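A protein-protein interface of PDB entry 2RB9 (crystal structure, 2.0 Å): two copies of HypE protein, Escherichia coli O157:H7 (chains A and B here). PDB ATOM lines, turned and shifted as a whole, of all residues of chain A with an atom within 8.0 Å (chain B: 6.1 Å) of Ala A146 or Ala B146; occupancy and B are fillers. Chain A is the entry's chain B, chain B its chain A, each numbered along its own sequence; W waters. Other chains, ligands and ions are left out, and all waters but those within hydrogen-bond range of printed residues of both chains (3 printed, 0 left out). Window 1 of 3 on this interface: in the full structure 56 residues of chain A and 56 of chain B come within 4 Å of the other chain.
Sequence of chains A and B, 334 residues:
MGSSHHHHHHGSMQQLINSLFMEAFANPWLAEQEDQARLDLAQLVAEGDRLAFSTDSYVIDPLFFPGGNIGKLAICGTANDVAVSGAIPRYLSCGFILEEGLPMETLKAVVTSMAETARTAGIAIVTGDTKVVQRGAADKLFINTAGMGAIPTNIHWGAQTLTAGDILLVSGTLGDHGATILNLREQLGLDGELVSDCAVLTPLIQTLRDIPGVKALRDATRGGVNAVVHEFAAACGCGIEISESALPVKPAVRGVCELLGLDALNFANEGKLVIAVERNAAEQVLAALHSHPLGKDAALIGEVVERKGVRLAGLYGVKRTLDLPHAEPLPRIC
Tyr A91 touches none of the printed residues of chain B.
Of the printed residues of chain B, Val A126 touches Phe B53 (3.7 Å).
Of the printed residues of chain B, Thr A127 touches Phe B53 (3.7 Å).
Of the printed residues of chain B, Asn A144 touches Asn B144.
Ala A146 touches just one residue of chain B: Ala B146 (3.9 Å).
Of the printed residues of chain A, Ser B93 touches Phe A53 (3.6 Å) and Thr A55 (3.7 Å).
Ala B146 touches just one residue of chain A: Ala A146 (3.9 Å).
The nearest residue of chain B that does not touch Ala A146 is Ser B93 (4.1 Å).
Hydrophobic or aromatic side chains of chain B that line the printed part of chain A: Phe B53, Ala B146 and Met B148.
Hydrophobic or aromatic side chains of chain A that line the printed part of chain B: Phe A53, Val A126, Ala A146 and Met A148.
Among the printed residues, 12 pairs touch across the chains.
Among the printed residues, no Asp or Glu carboxylate lies within 4 Å of a Lys or Arg side-chain nitrogen of the other chain.
Water W3 bridges OG1 of Thr A127 and N of Thr B55.
Water W2 lies within hydrogen-bond range of the side-chain hydroxyl (OG) of Ser B93 (2.7 Å), the side-chain hydroxyl (OG1) of Thr A55 (2.7 Å), the side-chain amide oxygen (OD1) of Asn B144 (3.0 Å) and the side-chain amide oxygen (OD1) of Asn A144 (3.4 Å).
Water W1 lies within hydrogen-bond range of OG1 of Thr B55 (2.8 Å), OG of Ser A93 (2.8 Å), OD1 of Asn A144 (2.9 Å) and OD1 of Asn B144 (3.4 Å).
Phe A53 touches Met B148, and with the chains exchanged Met A148 touches Phe B53.
Thr A55 touches Ser B93, and with the chains exchanged Ser A93 touches Thr B55.
Ala B146 touches its own counterpart, Ala A146.
Met B148 touches its own counterpart, Met A148.
Positions printed for both chains: 53, 54, 55, 56, 78, 91, 92, 93, 94, 144, 145, 146, 147 and 148.
Among the printed residues, merely in contact across the chains: Ser A93 with Phe B53 (3.6 Å), Phe A53 with Ser B93 (3.6 Å), Met A148 with Phe B53 (3.7 Å), Phe A53 with Met B148 (3.7 Å), Ser A93 with Thr B55 (3.7 Å), Thr A127 with Phe B53 (3.7 Å), Thr A55 with Ser B93 (3.7 Å), Val A126 with Phe B53 (3.7 Å), Met A148 with Met B148 (3.8 Å), Ala A146 with Ala B146 (3.9 Å) and Phe A53 with Phe B53 (3.96 Å).
The side-chain amide nitrogen (ND2) of Asn B144 lies within hydrogen-bond range of the backbone carbonyl oxygen (O) of Asp B56, 3.1 Å away.
The backbone NH (N) of Met B148 lies within hydrogen-bond range of the backbone carbonyl oxygen (O) of Tyr B91 (3.0 Å).
The backbone NH (N) of Ser B93 is in hydrogen-bond range of the backbone carbonyl oxygen (O) of Ala B146 (2.7 Å).
The backbone carbonyl oxygen of Thr A145 lies within hydrogen-bond range of the side-chain hydroxyl of Thr A55, 3.1 Å away.
O of Asp A56 sits at hydrogen-bond distance from ND2 of Asn A144 (3.2 Å).
O of Ala A146 is in hydrogen-bond range of N of Ser A93 (2.8 Å).
The side-chain amide oxygen of Asn A144 sits close to the side-chain amide oxygen of Asn B144.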
ATOM      1  N   ALA A  52     -11.204  17.245  17.823  1.00  0.00           N
ATOM      2  CA  ALA A  52     -10.175  16.242  18.139  1.00  0.00           C
ATOM      3  C   ALA A  52      -8.912  16.984  18.530  1.00  0.00           C
ATOM      4  O   ALA A  52      -8.529  17.929  17.857  1.00  0.00           O
ATOM      5  CB  ALA A  52      -9.893  15.368  16.935  1.00  0.00           C
ATOM      6  N   PHE A  53      -8.257  16.541  19.601  1.00  0.00           N
ATOM      7  CA  PHE A  53      -7.098  17.232  20.151  1.00  0.00           C
ATOM      8  C   PHE A  53      -6.137  16.175  20.676  1.00  0.00           C
ATOM      9  O   PHE A  53      -6.512  15.341  21.505  1.00  0.00           O
ATOM     10  CB  PHE A  53      -7.557  18.185  21.272  1.00  0.00           C
ATOM     11  CG  PHE A  53      -6.441  18.952  21.949  1.00  0.00           C
ATOM     12  CD1 PHE A  53      -5.470  19.626  21.210  1.00  0.00           C
ATOM     13  CD2 PHE A  53      -6.399  19.038  23.343  1.00  0.00           C
ATOM     14  CE1 PHE A  53      -4.446  20.349  21.850  1.00  0.00           C
ATOM     15  CE2 PHE A  53      -5.385  19.770  23.991  1.00  0.00           C
ATOM     16  CZ  PHE A  53      -4.408  20.423  23.232  1.00  0.00           C
ATOM     17  N   SER A  54      -4.908  16.190  20.162  1.00  0.00           N
ATOM     18  CA  SER A  54      -3.902  15.194  20.518  1.00  0.00           C
ATOM     19  C   SER A  54      -2.540  15.840  20.727  1.00  0.00           C
ATOM     20  O   SER A  54      -2.275  16.923  20.190  1.00  0.00           O
ATOM     21  CB  SER A  54      -3.788  14.162  19.402  1.00  0.00           C
ATOM     22  OG  SER A  54      -3.166  14.735  18.264  1.00  0.00           O
ATOM     23  N   THR A  55      -1.680  15.166  21.482  1.00  0.00           N
ATOM     24  CA  THR A  55      -0.305  15.610  21.653  1.00  0.00           C
ATOM     25  C   THR A  55       0.598  14.388  21.706  1.00  0.00           C
ATOM     26  O   THR A  55       0.167  13.322  22.156  1.00  0.00           O
ATOM     27  CB  THR A  55      -0.112  16.485  22.920  1.00  0.00           C
ATOM     28  OG1 THR A  55       1.181  17.103  22.878  1.00  0.00           O
ATOM     29  CG2 THR A  55      -0.234  15.659  24.208  1.00  0.00           C
ATOM     30  N   ASP A  56       1.829  14.544  21.225  1.00  0.00           N
ATOM     31  CA  ASP A  56       2.854  13.496  21.291  1.00  0.00           C
ATOM     32  C   ASP A  56       4.203  14.187  21.412  1.00  0.00           C
ATOM     33  O   ASP A  56       4.386  15.260  20.846  1.00  0.00           O
ATOM     34  CB  ASP A  56       2.872  12.665  20.004  1.00  0.00           C
ATOM     35  CG  ASP A  56       1.690  11.727  19.880  1.00  0.00           C
ATOM     36  OD1 ASP A  56       1.671  10.702  20.593  1.00  0.00           O
ATOM     37  OD2 ASP A  56       0.793  12.000  19.041  1.00  0.00           O
ATOM     38  N   SER A  57       5.135  13.577  22.144  1.00  0.00           N
ATOM     39  CA  SER A  57       6.532  14.011  22.145  1.00  0.00           C
ATOM     40  C   SER A  57       7.366  13.037  21.326  1.00  0.00           C
ATOM     41  O   SER A  57       7.040  11.850  21.226  1.00  0.00           O
ATOM     42  CB  SER A  57       7.099  14.117  23.562  1.00  0.00           C
ATOM     43  OG  SER A  57       6.462  15.155  24.293  1.00  0.00           O
ATOM     44  N   TYR A  58       8.442  13.550  20.747  1.00  0.00           N
ATOM     45  CA  TYR A  58       9.290  12.779  19.848  1.00  0.00           C
ATOM     46  C   TYR A  58      10.725  12.858  20.340  1.00  0.00           C
ATOM     47  O   TYR A  58      11.295  13.948  20.467  1.00  0.00           O
ATOM     48  CB  TYR A  58       9.118  13.274  18.403  1.00  0.00           C
ATOM     49  CG  TYR A  58       7.669  13.157  17.961  1.00  0.00           C
ATOM     50  CD1 TYR A  58       6.748  14.169  18.243  1.00  0.00           C
ATOM     51  CD2 TYR A  58       7.207  12.007  17.324  1.00  0.00           C
ATOM     52  CE1 TYR A  58       5.407  14.051  17.877  1.00  0.00           C
ATOM     53  CE2 TYR A  58       5.867  11.877  16.951  1.00  0.00           C
ATOM     54  CZ  TYR A  58       4.977  12.901  17.234  1.00  0.00           C
ATOM     55  OH  TYR A  58       3.656  12.784  16.870  1.00  0.00           O
ATOM     56  N   ALA A  74       7.313  14.175  13.761  1.00  0.00           N
ATOM     57  CA  ALA A  74       6.581  15.036  14.697  1.00  0.00           C
ATOM     58  C   ALA A  74       5.284  15.582  14.104  1.00  0.00           C
ATOM     59  O   ALA A  74       4.308  15.795  14.828  1.00  0.00           O
ATOM     60  CB  ALA A  74       7.468  16.181  15.184  1.00  0.00           C
ATOM     61  N   THR A  78       1.320  13.250  15.128  1.00  0.00           N
ATOM     62  CA  THR A  78       0.266  14.063  15.731  1.00  0.00           C
ATOM     63  C   THR A  78      -0.892  14.287  14.759  1.00  0.00           C
ATOM     64  O   THR A  78      -2.052  14.264  15.165  1.00  0.00           O
ATOM     65  CB  THR A  78       0.846  15.387  16.255  1.00  0.00           C
ATOM     66  OG1 THR A  78       1.774  15.083  17.303  1.00  0.00           O
ATOM     67  CG2 THR A  78      -0.245  16.310  16.795  1.00  0.00           C
ATOM     68  N   ALA A  79      -0.577  14.482  13.480  1.00  0.00           N
ATOM     69  CA  ALA A  79      -1.603  14.552  12.439  1.00  0.00           C
ATOM     70  C   ALA A  79      -2.437  13.274  12.445  1.00  0.00           C
ATOM     71  O   ALA A  79      -3.664  13.326  12.411  1.00  0.00           O
ATOM     72  CB  ALA A  79      -0.969  14.755  11.076  1.00  0.00           C
ATOM     73  N   VAL A  82      -4.924  12.838  15.342  1.00  0.00           N
ATOM     74  CA  VAL A  82      -6.130  13.629  15.041  1.00  0.00           C
ATOM     75  C   VAL A  82      -6.977  12.950  13.960  1.00  0.00           C
ATOM     76  O   VAL A  82      -8.189  12.761  14.130  1.00  0.00           O
ATOM     77  CB  VAL A  82      -5.766  15.081  14.619  1.00  0.00           C
ATOM     78  CG1 VAL A  82      -6.983  15.823  14.004  1.00  0.00           C
ATOM     79  CG2 VAL A  82      -5.208  15.856  15.812  1.00  0.00           C
ATOM     80  N   TYR A  91      -4.597  22.417  12.438  1.00  0.00           N
ATOM     81  CA  TYR A  91      -3.693  23.263  13.219  1.00  0.00           C
ATOM     82  C   TYR A  91      -2.817  22.448  14.153  1.00  0.00           C
ATOM     83  O   TYR A  91      -3.312  21.561  14.857  1.00  0.00           O
ATOM     84  CB  TYR A  91      -4.490  24.281  14.051  1.00  0.00           C
ATOM     85  CG  TYR A  91      -5.494  25.106  13.266  1.00  0.00           C
ATOM     86  CD1 TYR A  91      -6.852  25.086  13.594  1.00  0.00           C
ATOM     87  CD2 TYR A  91      -5.085  25.909  12.200  1.00  0.00           C
ATOM     88  CE1 TYR A  91      -7.778  25.848  12.885  1.00  0.00           C
ATOM     89  CE2 TYR A  91      -6.007  26.674  11.477  1.00  0.00           C
ATOM     90  CZ  TYR A  91      -7.349  26.638  11.829  1.00  0.00           C
ATOM     91  OH  TYR A  91      -8.263  27.390  11.117  1.00  0.00           O
ATOM     92  N   LEU A  92      -1.523  22.769  14.159  1.00  0.00           N
ATOM     93  CA  LEU A  92      -0.547  22.149  15.052  1.00  0.00           C
ATOM     94  C   LEU A  92       0.249  23.205  15.814  1.00  0.00           C
ATOM     95  O   LEU A  92       0.501  24.296  15.294  1.00  0.00           O
ATOM     96  CB  LEU A  92       0.423  21.239  14.272  1.00  0.00           C
ATOM     97  CG  LEU A  92       0.254  19.711  14.385  1.00  0.00           C
ATOM     98  CD1 LEU A  92      -1.099  19.248  13.857  1.00  0.00           C
ATOM     99  CD2 LEU A  92       1.376  18.960  13.675  1.00  0.00           C
ATOM    100  N   SER A  93       0.609  22.877  17.054  1.00  0.00           N
ATOM    101  CA  SER A  93       1.596  23.623  17.817  1.00  0.00           C
ATOM    102  C   SER A  93       2.887  22.815  17.809  1.00  0.00           C
ATOM    103  O   SER A  93       2.854  21.594  17.614  1.00  0.00           O
ATOM    104  CB  SER A  93       1.130  23.836  19.255  1.00  0.00           C
ATOM    105  OG  SER A  93       1.019  22.599  19.944  1.00  0.00           O
ATOM    106  N   CYS A  94       4.012  23.492  18.034  1.00  0.00           N
ATOM    107  CA  CYS A  94       5.323  22.857  17.985  1.00  0.00           C
ATOM    108  C   CYS A  94       6.258  23.378  19.081  1.00  0.00           C
ATOM    109  O   CYS A  94       6.569  24.566  19.124  1.00  0.00           O
ATOM    110  CB  CYS A  94       5.941  23.093  16.609  1.00  0.00           C
ATOM    111  SG  CYS A  94       7.583  22.411  16.423  1.00  0.00           S
ATOM    112  N   GLY A  95       6.701  22.492  19.966  1.00  0.00           N
ATOM    113  CA  GLY A  95       7.626  22.875  21.034  1.00  0.00           C
ATOM    114  C   GLY A  95       8.961  22.177  20.880  1.00  0.00           C
ATOM    115  O   GLY A  95       9.018  20.947  20.886  1.00  0.00           O
ATOM    116  N   ILE A 123      -1.636  21.503   6.723  1.00  0.00           N
ATOM    117  CA  ILE A 123      -1.645  21.782   8.152  1.00  0.00           C
ATOM    118  C   ILE A 123      -0.827  23.037   8.432  1.00  0.00           C
ATOM    119  O   ILE A 123       0.273  23.181   7.919  1.00  0.00           O
ATOM    120  CB  ILE A 123      -1.054  20.599   8.952  1.00  0.00           C
ATOM    121  CG1 ILE A 123      -1.937  19.358   8.793  1.00  0.00           C
ATOM    122  CG2 ILE A 123      -0.894  20.959  10.438  1.00  0.00           C
ATOM    123  CD1 ILE A 123      -1.291  18.076   9.296  1.00  0.00           C
ATOM    124  N   ALA A 124      -1.383  23.939   9.237  1.00  0.00           N
ATOM    125  CA  ALA A 124      -0.686  25.149   9.645  1.00  0.00           C
ATOM    126  C   ALA A 124      -0.096  24.971  11.037  1.00  0.00           C
ATOM    127  O   ALA A 124      -0.795  24.554  11.968  1.00  0.00           O
ATOM    128  CB  ALA A 124      -1.639  26.344   9.624  1.00  0.00           C
ATOM    129  N   ILE A 125       1.191  25.279  11.166  1.00  0.00           N
ATOM    130  CA  ILE A 125       1.841  25.342  12.472  1.00  0.00           C
ATOM    131  C   ILE A 125       1.614  26.761  13.004  1.00  0.00           C
ATOM    132  O   ILE A 125       2.259  27.717  12.557  1.00  0.00           O
ATOM    133  CB  ILE A 125       3.343  24.970  12.392  1.00  0.00           C
ATOM    134  CG1 ILE A 125       3.503  23.565  11.797  1.00  0.00           C
ATOM    135  CG2 ILE A 125       4.006  25.062  13.771  1.00  0.00           C
ATOM    136  CD1 ILE A 125       4.921  23.202  11.399  1.00  0.00           C
ATOM    137  N   VAL A 126       0.680  26.878  13.947  1.00  0.00           N
ATOM    138  CA  VAL A 126       0.105  28.171  14.333  1.00  0.00           C
ATOM    139  C   VAL A 126       0.745  28.806  15.560  1.00  0.00           C
ATOM    140  O   VAL A 126       0.542  29.989  15.832  1.00  0.00           O
ATOM    141  CB  VAL A 126      -1.429  28.078  14.545  1.00  0.00           C
ATOM    142  CG1 VAL A 126      -2.116  27.700  13.239  1.00  0.00           C
ATOM    143  CG2 VAL A 126      -1.784  27.084  15.668  1.00  0.00           C
ATOM    144  N   THR A 127       1.502  28.013  16.305  1.00  0.00           N
ATOM    145  CA  THR A 127       2.125  28.491  17.524  1.00  0.00           C
ATOM    146  C   THR A 127       3.239  27.544  17.948  1.00  0.00           C
ATOM    147  O   THR A 127       3.312  26.401  17.486  1.00  0.00           O
ATOM    148  CB  THR A 127       1.080  28.732  18.663  1.00  0.00           C
ATOM    149  OG1 THR A 127       1.654  29.567  19.672  1.00  0.00           O
ATOM    150  CG2 THR A 127       0.581  27.432  19.283  1.00  0.00           C
ATOM    151  N   ILE A 143      11.099  17.038  20.309  1.00  0.00           N
ATOM    152  CA  ILE A 143       9.987  17.848  19.794  1.00  0.00           C
ATOM    153  C   ILE A 143       8.669  17.396  20.413  1.00  0.00           C
ATOM    154  O   ILE A 143       8.398  16.196  20.485  1.00  0.00           O
ATOM    155  CB  ILE A 143       9.845  17.732  18.248  1.00  0.00           C
ATOM    156  CG1 ILE A 143      11.194  17.925  17.541  1.00  0.00           C
ATOM    157  CG2 ILE A 143       8.805  18.732  17.716  1.00  0.00           C
ATOM    158  CD1 ILE A 143      11.161  17.648  16.041  1.00  0.00           C
ATOM    159  N   ASN A 144       7.856  18.347  20.866  1.00  0.00           N
ATOM    160  CA  ASN A 144       6.452  18.060  21.145  1.00  0.00           C
ATOM    161  C   ASN A 144       5.564  18.787  20.147  1.00  0.00           C
ATOM    162  O   ASN A 144       5.798  19.958  19.839  1.00  0.00           O
ATOM    163  CB  ASN A 144       6.057  18.446  22.571  1.00  0.00           C
ATOM    164  CG  ASN A 144       4.583  18.173  22.862  1.00  0.00           C
ATOM    165  OD1 ASN A 144       3.698  18.968  22.501  1.00  0.00           O
ATOM    166  ND2 ASN A 144       4.310  17.040  23.506  1.00  0.00           N
ATOM    167  N   THR A 145       4.562  18.083  19.627  1.00  0.00           N
ATOM    168  CA  THR A 145       3.523  18.725  18.831  1.00  0.00           C
ATOM    169  C   THR A 145       2.155  18.380  19.388  1.00  0.00           C
ATOM    170  O   THR A 145       1.939  17.270  19.892  1.00  0.00           O
ATOM    171  CB  THR A 145       3.557  18.325  17.342  1.00  0.00           C
ATOM    172  OG1 THR A 145       3.570  16.896  17.228  1.00  0.00           O
ATOM    173  CG2 THR A 145       4.782  18.916  16.633  1.00  0.00           C
ATOM    174  N   ALA A 146       1.240  19.338  19.296  1.00  0.00           N
ATOM    175  CA  ALA A 146      -0.159  19.108  19.609  1.00  0.00           C
ATOM    176  C   ALA A 146      -0.983  19.548  18.407  1.00  0.00           C
ATOM    177  O   ALA A 146      -0.615  20.494  17.709  1.00  0.00           O
ATOM    178  CB  ALA A 146      -0.564  19.865  20.870  1.00  0.00           C
ATOM    179  N   GLY A 147      -2.078  18.852  18.136  1.00  0.00           N
ATOM    180  CA  GLY A 147      -2.829  19.134  16.921  1.00  0.00           C
ATOM    181  C   GLY A 147      -4.316  19.032  17.114  1.00  0.00           C
ATOM    182  O   GLY A 147      -4.784  18.404  18.059  1.00  0.00           O
ATOM    183  N   MET A 148      -5.062  19.628  16.192  1.00  0.00           N
ATOM    184  CA  MET A 148      -6.508  19.619  16.284  1.00  0.00           C
ATOM    185  C   MET A 148      -7.187  19.651  14.921  1.00  0.00           C
ATOM    186  O   MET A 148      -6.603  20.051  13.920  1.00  0.00           O
ATOM    187  CB  MET A 148      -7.004  20.781  17.156  1.00  0.00           C
ATOM    188  CG  MET A 148      -6.799  22.150  16.524  1.00  0.00           C
ATOM    189  SD  MET A 148      -7.382  23.503  17.563  1.00  0.00           S
ATOM    190  CE  MET A 148      -6.156  23.511  18.852  1.00  0.00           C
ATOM    191  N   PHE B  53      -5.028  29.380  21.591  1.00  0.00           N
ATOM    192  CA  PHE B  53      -4.264  28.139  21.567  1.00  0.00           C
ATOM    193  C   PHE B  53      -2.785  28.468  21.716  1.00  0.00           C
ATOM    194  O   PHE B  53      -2.228  29.228  20.916  1.00  0.00           O
ATOM    195  CB  PHE B  53      -4.540  27.393  20.252  1.00  0.00           C
ATOM    196  CG  PHE B  53      -3.775  26.102  20.095  1.00  0.00           C
ATOM    197  CD1 PHE B  53      -3.752  25.150  21.120  1.00  0.00           C
ATOM    198  CD2 PHE B  53      -3.122  25.820  18.903  1.00  0.00           C
ATOM    199  CE1 PHE B  53      -3.045  23.948  20.967  1.00  0.00           C
ATOM    200  CE2 PHE B  53      -2.421  24.615  18.730  1.00  0.00           C
ATOM    201  CZ  PHE B  53      -2.389  23.678  19.769  1.00  0.00           C
ATOM    202  N   SER B  54      -2.156  27.921  22.755  1.00  0.00           N
ATOM    203  CA  SER B  54      -0.740  28.166  23.004  1.00  0.00           C
ATOM    204  C   SER B  54      -0.016  26.904  23.457  1.00  0.00           C
ATOM    205  O   SER B  54      -0.643  25.942  23.898  1.00  0.00           O
ATOM    206  CB  SER B  54      -0.573  29.263  24.055  1.00  0.00           C
ATOM    207  OG  SER B  54      -1.022  28.809  25.321  1.00  0.00           O
ATOM    208  N   THR B  55       1.307  26.923  23.345  1.00  0.00           N
ATOM    209  CA  THR B  55       2.135  25.850  23.870  1.00  0.00           C
ATOM    210  C   THR B  55       3.423  26.409  24.468  1.00  0.00           C
ATOM    211  O   THR B  55       3.933  27.443  24.018  1.00  0.00           O
ATOM    212  CB  THR B  55       2.463  24.794  22.795  1.00  0.00           C
ATOM    213  OG1 THR B  55       3.083  23.661  23.421  1.00  0.00           O
ATOM    214  CG2 THR B  55       3.407  25.373  21.729  1.00  0.00           C
ATOM    215  N   ASP B  56       3.937  25.730  25.488  1.00  0.00           N
ATOM    216  CA  ASP B  56       5.234  26.068  26.062  1.00  0.00           C
ATOM    217  C   ASP B  56       5.867  24.800  26.604  1.00  0.00           C
ATOM    218  O   ASP B  56       5.162  23.873  27.027  1.00  0.00           O
ATOM    219  CB  ASP B  56       5.088  27.111  27.183  1.00  0.00           C
ATOM    220  CG  ASP B  56       6.382  27.895  27.443  1.00  0.00           C
ATOM    221  OD1 ASP B  56       7.140  28.170  26.492  1.00  0.00           O
ATOM    222  OD2 ASP B  56       6.636  28.265  28.610  1.00  0.00           O
ATOM    223  N   THR B  78       1.131  27.997  30.796  1.00  0.00           N
ATOM    224  CA  THR B  78       0.309  27.744  29.625  1.00  0.00           C
ATOM    225  C   THR B  78      -1.117  28.249  29.848  1.00  0.00           C
ATOM    226  O   THR B  78      -1.714  28.819  28.939  1.00  0.00           O
ATOM    227  CB  THR B  78       0.370  26.254  29.223  1.00  0.00           C
ATOM    228  OG1 THR B  78       1.703  25.962  28.782  1.00  0.00           O
ATOM    229  CG2 THR B  78      -0.611  25.933  28.091  1.00  0.00           C
ATOM    230  N   TYR B  91      -8.986  23.459  28.596  1.00  0.00           N
ATOM    231  CA  TYR B  91      -8.395  22.174  28.245  1.00  0.00           C
ATOM    232  C   TYR B  91      -6.907  22.294  27.972  1.00  0.00           C
ATOM    233  O   TYR B  91      -6.478  23.166  27.212  1.00  0.00           O
ATOM    234  CB  TYR B  91      -9.091  21.586  27.016  1.00  0.00           C
ATOM    235  CG  TYR B  91     -10.604  21.554  27.088  1.00  0.00           C
ATOM    236  CD1 TYR B  91     -11.369  22.284  26.182  1.00  0.00           C
ATOM    237  CD2 TYR B  91     -11.267  20.784  28.048  1.00  0.00           C
ATOM    238  CE1 TYR B  91     -12.759  22.251  26.221  1.00  0.00           C
ATOM    239  CE2 TYR B  91     -12.666  20.743  28.100  1.00  0.00           C
ATOM    240  CZ  TYR B  91     -13.399  21.482  27.179  1.00  0.00           C
ATOM    241  OH  TYR B  91     -14.776  21.452  27.205  1.00  0.00           O
ATOM    242  N   LEU B  92      -6.131  21.420  28.610  1.00  0.00           N
ATOM    243  CA  LEU B  92      -4.683  21.364  28.415  1.00  0.00           C
ATOM    244  C   LEU B  92      -4.221  19.970  27.992  1.00  0.00           C
ATOM    245  O   LEU B  92      -4.846  18.964  28.342  1.00  0.00           O
ATOM    246  CB  LEU B  92      -3.944  21.797  29.691  1.00  0.00           C
ATOM    247  CG  LEU B  92      -3.366  23.219  29.738  1.00  0.00           C
ATOM    248  CD1 LEU B  92      -4.471  24.277  29.725  1.00  0.00           C
ATOM    249  CD2 LEU B  92      -2.473  23.386  30.964  1.00  0.00           C
ATOM    250  N   SER B  93      -3.136  19.934  27.225  1.00  0.00           N
ATOM    251  CA  SER B  93      -2.435  18.696  26.895  1.00  0.00           C
ATOM    252  C   SER B  93      -1.099  18.703  27.622  1.00  0.00           C
ATOM    253  O   SER B  93      -0.604  19.766  27.995  1.00  0.00           O
ATOM    254  CB  SER B  93      -2.230  18.563  25.386  1.00  0.00           C
ATOM    255  OG  SER B  93      -1.314  19.526  24.888  1.00  0.00           O
ATOM    256  N   CYS B  94      -0.520  17.524  27.828  1.00  0.00           N
ATOM    257  CA  CYS B  94       0.711  17.406  28.605  1.00  0.00           C
ATOM    258  C   CYS B  94       1.642  16.306  28.087  1.00  0.00           C
ATOM    259  O   CYS B  94       1.268  15.133  28.036  1.00  0.00           O
ATOM    260  CB  CYS B  94       0.374  17.163  30.074  1.00  0.00           C
ATOM    261  SG  CYS B  94       1.809  16.896  31.112  1.00  0.00           S
ATOM    262  N   ASN B 144       6.065  19.567  28.296  1.00  0.00           N
ATOM    263  CA  ASN B 144       5.382  20.477  27.384  1.00  0.00           C
ATOM    264  C   ASN B 144       3.893  20.461  27.666  1.00  0.00           C
ATOM    265  O   ASN B 144       3.296  19.395  27.845  1.00  0.00           O
ATOM    266  CB  ASN B 144       5.647  20.132  25.912  1.00  0.00           C
ATOM    267  CG  ASN B 144       4.869  21.035  24.959  1.00  0.00           C
ATOM    268  OD1 ASN B 144       3.686  20.797  24.681  1.00  0.00           O
ATOM    269  ND2 ASN B 144       5.524  22.088  24.471  1.00  0.00           N
ATOM    270  N   THR B 145       3.292  21.644  27.740  1.00  0.00           N
ATOM    271  CA  THR B 145       1.843  21.725  27.804  1.00  0.00           C
ATOM    272  C   THR B 145       1.345  22.620  26.684  1.00  0.00           C
ATOM    273  O   THR B 145       2.005  23.593  26.315  1.00  0.00           O
ATOM    274  CB  THR B 145       1.318  22.220  29.180  1.00  0.00           C
ATOM    275  OG1 THR B 145       1.959  23.450  29.535  1.00  0.00           O
ATOM    276  CG2 THR B 145       1.575  21.177  30.278  1.00  0.00           C
ATOM    277  N   ALA B 146       0.199  22.263  26.123  1.00  0.00           N
ATOM    278  CA  ALA B 146      -0.502  23.115  25.167  1.00  0.00           C
ATOM    279  C   ALA B 146      -1.892  23.318  25.726  1.00  0.00           C
ATOM    280  O   ALA B 146      -2.424  22.432  26.397  1.00  0.00           O
ATOM    281  CB  ALA B 146      -0.569  22.467  23.798  1.00  0.00           C
ATOM    282  N   GLY B 147      -2.483  24.476  25.457  1.00  0.00           N
ATOM    283  CA  GLY B 147      -3.749  24.823  26.092  1.00  0.00           C
ATOM    284  C   GLY B 147      -4.684  25.615  25.220  1.00  0.00           C
ATOM    285  O   GLY B 147      -4.262  26.243  24.239  1.00  0.00           O
ATOM    286  N   MET B 148      -5.959  25.606  25.585  1.00  0.00           N
ATOM    287  CA  MET B 148      -6.959  26.321  24.797  1.00  0.00           C
ATOM    288  C   MET B 148      -8.118  26.853  25.629  1.00  0.00           C
ATOM    289  O   MET B 148      -8.412  26.346  26.714  1.00  0.00           O
ATOM    290  CB  MET B 148      -7.490  25.434  23.663  1.00  0.00           C
ATOM    291  CG  MET B 148      -8.394  24.297  24.143  1.00  0.00           C
ATOM    292  SD  MET B 148      -9.028  23.313  22.776  1.00  0.00           S
ATOM    293  CE  MET B 148      -7.525  22.525  22.212  1.00  0.00           C
HETATM  294  O   HOH W   1       3.233  21.683  21.450  1.00  0.00           O
HETATM  295  O   HOH W   2       1.326  18.953  24.886  1.00  0.00           O
HETATM  296  O   HOH W   3       2.406  29.507  22.164  1.00  0.00           O
